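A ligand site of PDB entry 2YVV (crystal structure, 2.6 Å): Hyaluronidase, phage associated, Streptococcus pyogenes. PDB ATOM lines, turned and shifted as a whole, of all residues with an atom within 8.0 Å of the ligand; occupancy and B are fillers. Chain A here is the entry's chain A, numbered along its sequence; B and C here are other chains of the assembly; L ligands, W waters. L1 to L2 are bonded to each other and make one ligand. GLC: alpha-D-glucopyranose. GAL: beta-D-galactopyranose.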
ATOM      1  N   ARG A 163       3.608   3.348   4.020  1.00  0.00           N
ATOM      2  CA  ARG A 163       3.773   1.988   3.468  1.00  0.00           C
ATOM      3  C   ARG A 163       5.082   1.336   3.944  1.00  0.00           C
ATOM      4  O   ARG A 163       6.150   1.956   3.927  1.00  0.00           O
ATOM      5  CB  ARG A 163       3.713   2.015   1.930  1.00  0.00           C
ATOM      6  CG  ARG A 163       3.547   0.615   1.222  1.00  0.00           C
ATOM      7  CD  ARG A 163       3.808   0.632  -0.318  1.00  0.00           C
ATOM      8  NE  ARG A 163       5.097   1.291  -0.634  1.00  0.00           N
ATOM      9  CZ  ARG A 163       6.292   0.691  -0.640  1.00  0.00           C
ATOM     10  NH1 ARG A 163       6.384  -0.604  -0.345  1.00  0.00           N
ATOM     11  NH2 ARG A 163       7.404   1.361  -0.915  1.00  0.00           N
ATOM     12  N   THR A 164       4.983   0.095   4.389  1.00  0.00           N
ATOM     13  CA  THR A 164       6.192  -0.682   4.624  1.00  0.00           C
ATOM     14  C   THR A 164       6.181  -1.955   3.776  1.00  0.00           C
ATOM     15  O   THR A 164       5.170  -2.676   3.715  1.00  0.00           O
ATOM     16  CB  THR A 164       6.342  -1.047   6.080  1.00  0.00           C
ATOM     17  OG1 THR A 164       5.148  -1.721   6.524  1.00  0.00           O
ATOM     18  CG2 THR A 164       6.602   0.224   6.870  1.00  0.00           C
ATOM     19  N   GLY A 165       7.298  -2.238   3.113  1.00  0.00           N
ATOM     20  CA  GLY A 165       7.328  -3.290   2.105  1.00  0.00           C
ATOM     21  C   GLY A 165       7.865  -4.659   2.549  1.00  0.00           C
ATOM     22  O   GLY A 165       7.673  -5.629   1.850  1.00  0.00           O
ATOM     23  N   LYS A 166       8.507  -4.761   3.698  1.00  0.00           N
ATOM     24  CA  LYS A 166       9.146  -6.053   4.061  1.00  0.00           C
ATOM     25  C   LYS A 166       8.562  -6.675   5.307  1.00  0.00           C
ATOM     26  O   LYS A 166       8.421  -6.027   6.316  1.00  0.00           O
ATOM     27  CB  LYS A 166      10.665  -5.887   4.273  1.00  0.00           C
ATOM     28  CG  LYS A 166      11.464  -5.422   3.071  1.00  0.00           C
ATOM     29  CD  LYS A 166      12.118  -6.587   2.345  1.00  0.00           C
ATOM     30  CE  LYS A 166      11.479  -6.861   0.994  1.00  0.00           C
ATOM     31  NZ  LYS A 166      11.927  -6.078  -0.191  1.00  0.00           N
ATOM     32  N   GLU A 167       8.322  -7.975   5.260  1.00  0.00           N
ATOM     33  CA  GLU A 167       7.693  -8.656   6.375  1.00  0.00           C
ATOM     34  C   GLU A 167       8.451  -8.707   7.687  1.00  0.00           C
ATOM     35  O   GLU A 167       7.889  -9.010   8.742  1.00  0.00           O
ATOM     36  CB  GLU A 167       7.233 -10.030   5.921  1.00  0.00           C
ATOM     37  CG  GLU A 167       5.714 -10.020   5.585  1.00  0.00           C
ATOM     38  CD  GLU A 167       4.836  -9.629   6.827  1.00  0.00           C
ATOM     39  OE1 GLU A 167       4.965 -10.300   7.882  1.00  0.00           O
ATOM     40  OE2 GLU A 167       4.034  -8.653   6.743  1.00  0.00           O
ATOM     41  N   TYR B 149       7.529   5.872   3.041  1.00  0.00           N
ATOM     42  CA  TYR B 149       7.536   4.426   2.963  1.00  0.00           C
ATOM     43  C   TYR B 149       8.902   3.901   3.170  1.00  0.00           C
ATOM     44  O   TYR B 149       9.905   4.622   3.056  1.00  0.00           O
ATOM     45  CB  TYR B 149       7.048   3.958   1.597  1.00  0.00           C
ATOM     46  CG  TYR B 149       7.825   4.632   0.517  1.00  0.00           C
ATOM     47  CD1 TYR B 149       7.548   5.963   0.169  1.00  0.00           C
ATOM     48  CD2 TYR B 149       8.888   3.984  -0.118  1.00  0.00           C
ATOM     49  CE1 TYR B 149       8.294   6.625  -0.811  1.00  0.00           C
ATOM     50  CE2 TYR B 149       9.637   4.632  -1.116  1.00  0.00           C
ATOM     51  CZ  TYR B 149       9.329   5.954  -1.453  1.00  0.00           C
ATOM     52  OH  TYR B 149      10.050   6.627  -2.411  1.00  0.00           O
ATOM     53  N   SER B 150       8.971   2.619   3.447  1.00  0.00           N
ATOM     54  CA  SER B 150      10.243   1.999   3.582  1.00  0.00           C
ATOM     55  C   SER B 150      10.154   0.594   3.057  1.00  0.00           C
ATOM     56  O   SER B 150       9.163  -0.120   3.318  1.00  0.00           O
ATOM     57  CB  SER B 150      10.642   1.955   5.041  1.00  0.00           C
ATOM     58  OG  SER B 150      11.816   1.152   5.182  1.00  0.00           O
ATOM     59  N   ASP B 151      11.181   0.209   2.293  1.00  0.00           N
ATOM     60  CA  ASP B 151      11.358  -1.180   1.907  1.00  0.00           C
ATOM     61  C   ASP B 151      12.572  -1.821   2.578  1.00  0.00           C
ATOM     62  O   ASP B 151      13.120  -2.794   2.101  1.00  0.00           O
ATOM     63  CB  ASP B 151      11.392  -1.288   0.397  1.00  0.00           C
ATOM     64  CG  ASP B 151      10.023  -0.980  -0.196  1.00  0.00           C
ATOM     65  OD1 ASP B 151       9.092  -1.798   0.036  1.00  0.00           O
ATOM     66  OD2 ASP B 151       9.853   0.103  -0.844  1.00  0.00           O
ATOM     67  N   ASN B 152      12.964  -1.271   3.724  1.00  0.00           N
ATOM     68  CA  ASN B 152      14.093  -1.769   4.488  1.00  0.00           C
ATOM     69  C   ASN B 152      13.680  -2.978   5.308  1.00  0.00           C
ATOM     70  O   ASN B 152      12.500  -3.167   5.597  1.00  0.00           O
ATOM     71  CB  ASN B 152      14.615  -0.680   5.384  1.00  0.00           C
ATOM     72  CG  ASN B 152      16.098  -0.826   5.658  1.00  0.00           C
ATOM     73  OD1 ASN B 152      16.695  -1.826   5.267  1.00  0.00           O
ATOM     74  ND2 ASN B 152      16.698   0.169   6.332  1.00  0.00           N
ATOM     75  N   ASP B 153      14.622  -3.816   5.667  1.00  0.00           N
ATOM     76  CA  ASP B 153      14.237  -5.053   6.303  1.00  0.00           C
ATOM     77  C   ASP B 153      13.867  -4.793   7.736  1.00  0.00           C
ATOM     78  O   ASP B 153      12.968  -5.433   8.273  1.00  0.00           O
ATOM     79  CB  ASP B 153      15.386  -6.047   6.274  1.00  0.00           C
ATOM     80  CG  ASP B 153      15.920  -6.239   4.891  1.00  0.00           C
ATOM     81  OD1 ASP B 153      15.179  -6.819   4.045  1.00  0.00           O
ATOM     82  OD2 ASP B 153      17.060  -5.777   4.646  1.00  0.00           O
ATOM     83  N   ARG B 190      -1.609  -6.459   5.534  1.00  0.00           N
ATOM     84  CA  ARG B 190      -1.487  -7.469   4.473  1.00  0.00           C
ATOM     85  C   ARG B 190      -1.166  -8.857   4.995  1.00  0.00           C
ATOM     86  O   ARG B 190      -0.334  -9.001   5.868  1.00  0.00           O
ATOM     87  CB  ARG B 190      -0.338  -7.029   3.530  1.00  0.00           C
ATOM     88  CG  ARG B 190      -0.446  -5.551   3.022  1.00  0.00           C
ATOM     89  CD  ARG B 190      -1.481  -5.541   1.898  1.00  0.00           C
ATOM     90  NE  ARG B 190      -1.791  -4.212   1.356  1.00  0.00           N
ATOM     91  CZ  ARG B 190      -3.013  -3.852   0.952  1.00  0.00           C
ATOM     92  NH1 ARG B 190      -4.024  -4.709   1.073  1.00  0.00           N
ATOM     93  NH2 ARG B 190      -3.230  -2.642   0.456  1.00  0.00           N
ATOM     94  N   SER C 129       4.580   4.574  -4.403  1.00  0.00           N
ATOM     95  CA  SER C 129       5.828   4.927  -3.694  1.00  0.00           C
ATOM     96  C   SER C 129       6.778   5.875  -4.486  1.00  0.00           C
ATOM     97  O   SER C 129       8.007   5.789  -4.361  1.00  0.00           O
ATOM     98  CB  SER C 129       6.580   3.660  -3.235  1.00  0.00           C
ATOM     99  OG  SER C 129       7.109   2.912  -4.315  1.00  0.00           O
ATOM    100  N   THR C 130       6.193   6.775  -5.275  1.00  0.00           N
ATOM    101  CA  THR C 130       6.981   7.760  -6.035  1.00  0.00           C
ATOM    102  C   THR C 130       6.190   9.077  -6.272  1.00  0.00           C
ATOM    103  O   THR C 130       6.648   9.986  -7.002  1.00  0.00           O
ATOM    104  CB  THR C 130       7.592   7.134  -7.352  1.00  0.00           C
ATOM    105  OG1 THR C 130       8.288   8.136  -8.114  1.00  0.00           O
ATOM    106  CG2 THR C 130       6.520   6.494  -8.217  1.00  0.00           C
ATOM    107  N   ASP C 137      11.622   8.289   1.477  1.00  0.00           N
ATOM    108  CA  ASP C 137      11.975   6.906   1.211  1.00  0.00           C
ATOM    109  C   ASP C 137      13.021   6.523   2.244  1.00  0.00           C
ATOM    110  O   ASP C 137      14.167   7.006   2.180  1.00  0.00           O
ATOM    111  CB  ASP C 137      12.567   6.783  -0.192  1.00  0.00           C
ATOM    112  CG  ASP C 137      13.025   5.361  -0.536  1.00  0.00           C
ATOM    113  OD1 ASP C 137      12.999   4.445   0.325  1.00  0.00           O
ATOM    114  OD2 ASP C 137      13.406   5.148  -1.697  1.00  0.00           O
ATOM    115  N   SER C 139      14.007   3.375   2.737  1.00  0.00           N
ATOM    116  CA  SER C 139      14.509   2.054   2.350  1.00  0.00           C
ATOM    117  C   SER C 139      15.967   1.732   2.662  1.00  0.00           C
ATOM    118  O   SER C 139      16.300   0.576   2.830  1.00  0.00           O
ATOM    119  CB  SER C 139      14.228   1.760   0.876  1.00  0.00           C
ATOM    120  OG  SER C 139      12.841   1.837   0.630  1.00  0.00           O
ATOM    121  N   ASP C 177      -0.560   1.060   4.710  1.00  0.00           N
ATOM    122  CA  ASP C 177      -0.366  -0.214   4.022  1.00  0.00           C
ATOM    123  C   ASP C 177       0.841  -0.860   4.696  1.00  0.00           C
ATOM    124  O   ASP C 177       1.989  -0.458   4.472  1.00  0.00           O
ATOM    125  CB  ASP C 177      -0.090   0.078   2.547  1.00  0.00           C
ATOM    126  CG  ASP C 177       0.034  -1.183   1.670  1.00  0.00           C
ATOM    127  OD1 ASP C 177      -0.056  -2.314   2.194  1.00  0.00           O
ATOM    128  OD2 ASP C 177       0.213  -1.032   0.429  1.00  0.00           O
ATOM    129  N   TYR C 178       0.614  -1.840   5.551  1.00  0.00           N
ATOM    130  CA  TYR C 178       1.698  -2.226   6.450  1.00  0.00           C
ATOM    131  C   TYR C 178       2.090  -3.663   6.310  1.00  0.00           C
ATOM    132  O   TYR C 178       1.237  -4.525   6.343  1.00  0.00           O
ATOM    133  CB  TYR C 178       1.296  -2.039   7.893  1.00  0.00           C
ATOM    134  CG  TYR C 178       2.357  -2.424   8.876  1.00  0.00           C
ATOM    135  CD1 TYR C 178       3.413  -1.553   9.175  1.00  0.00           C
ATOM    136  CD2 TYR C 178       2.294  -3.658   9.553  1.00  0.00           C
ATOM    137  CE1 TYR C 178       4.389  -1.899  10.128  1.00  0.00           C
ATOM    138  CE2 TYR C 178       3.270  -4.012  10.518  1.00  0.00           C
ATOM    139  CZ  TYR C 178       4.312  -3.117  10.806  1.00  0.00           C
ATOM    140  OH  TYR C 178       5.290  -3.420  11.753  1.00  0.00           O
ATOM    141  N   LYS C 179       3.394  -3.900   6.219  1.00  0.00           N
ATOM    142  CA  LYS C 179       3.979  -5.247   6.394  1.00  0.00           C
ATOM    143  C   LYS C 179       5.007  -5.125   7.484  1.00  0.00           C
ATOM    144  O   LYS C 179       5.710  -4.143   7.503  1.00  0.00           O
ATOM    145  CB  LYS C 179       4.639  -5.754   5.112  1.00  0.00           C
ATOM    146  CG  LYS C 179       3.612  -6.015   4.061  1.00  0.00           C
ATOM    147  CD  LYS C 179       4.098  -6.875   2.917  1.00  0.00           C
ATOM    148  CE  LYS C 179       3.158  -6.671   1.702  1.00  0.00           C
ATOM    149  NZ  LYS C 179       3.530  -7.576   0.576  1.00  0.00           N
HETATM  150  C1  GLC L   1       6.026  -5.381  -2.533  1.00  0.00           C
HETATM  151  C2  GLC L   1       6.908  -5.752  -1.366  1.00  0.00           C
HETATM  152  C3  GLC L   1       8.295  -4.951  -1.514  1.00  0.00           C
HETATM  153  C4  GLC L   1       8.958  -5.429  -2.820  1.00  0.00           C
HETATM  154  C5  GLC L   1       7.995  -5.164  -4.031  1.00  0.00           C
HETATM  155  C6  GLC L   1       8.616  -5.697  -5.365  1.00  0.00           C
HETATM  156  O1  GLC L   1       5.842  -3.938  -2.456  1.00  0.00           O
HETATM  157  O2  GLC L   1       6.212  -5.379  -0.170  1.00  0.00           O
HETATM  158  O3  GLC L   1       9.186  -5.250  -0.418  1.00  0.00           O
HETATM  159  O4  GLC L   1      10.293  -4.967  -3.299  1.00  0.00           O
HETATM  160  O5  GLC L   1       6.666  -5.784  -3.793  1.00  0.00           O
HETATM  161  O6  GLC L   1       7.712  -5.476  -6.451  1.00  0.00           O
HETATM  162  C1  GAL L   2      11.072  -3.728  -2.982  1.00  0.00           C
HETATM  163  C2  GAL L   2      12.405  -4.077  -3.751  1.00  0.00           C
HETATM  164  C3  GAL L   2      13.442  -2.973  -3.666  1.00  0.00           C
HETATM  165  C4  GAL L   2      12.726  -1.688  -4.253  1.00  0.00           C
HETATM  166  C5  GAL L   2      11.395  -1.296  -3.490  1.00  0.00           C
HETATM  167  C6  GAL L   2      10.766  -0.043  -4.244  1.00  0.00           C
HETATM  168  O2  GAL L   2      12.982  -5.270  -3.204  1.00  0.00           O
HETATM  169  O3  GAL L   2      14.665  -3.394  -4.452  1.00  0.00           O
HETATM  170  O4  GAL L   2      12.479  -1.853  -5.678  1.00  0.00           O
HETATM  171  O5  GAL L   2      10.517  -2.500  -3.631  1.00  0.00           O
HETATM  172  O6  GAL L   2      10.685   1.171  -3.463  1.00  0.00           O
HETATM  173  O   HOH W   1       3.408  -3.157  -2.549  1.00  0.00           O
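An oxygen (O6) of GAL L2 lies within hydrogen-bond range of the side-chain carboxylate of Asp 151 of chain B (2.9 Å). The backbone carbonyl oxygen of Gly 165 sits at hydrogen-bond distance from an oxygen (O2) of GLC L1 (2.5 Å). O3 of GLC L1 lies within hydrogen-bond range of NZ of Lys 166.
O of Arg 163 sits at hydrogen-bond distance from N of Ser 150 of chain B (2.9 Å). The backbone carbonyl oxygen (O) of Lys 179 of chain C sits at hydrogen-bond distance from the side-chain hydroxyl (OG1) of Thr 164 (2.7 Å). The backbone carbonyl oxygen (O) of Ser 150 of chain B is in hydrogen-bond range of the backbone NH (N) of Gly 165 (2.8 Å). The backbone NH of Asp 151 of chain B is in hydrogen-bond range of the side-chain hydroxyl of Ser 139 of chain C. The side-chain carboxylate (OD2) of Asp 151 of chain B lies within salt-bridge range of the guanidinium group (NH2) of Arg 163 (2.8 Å).
Residues that only touch the ligand: Lys 179 of chain C (3.5 Å) and Arg 163 (3.98 Å). Five residues have an atom within 4 Å of the ligand: Arg 163, Gly 165, Lys 166, Asp 151 of chain B and Lys 179 of chain C. The nearest printed residue that does not touch the ligand is Ser 129 of chain C (4.1 Å).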
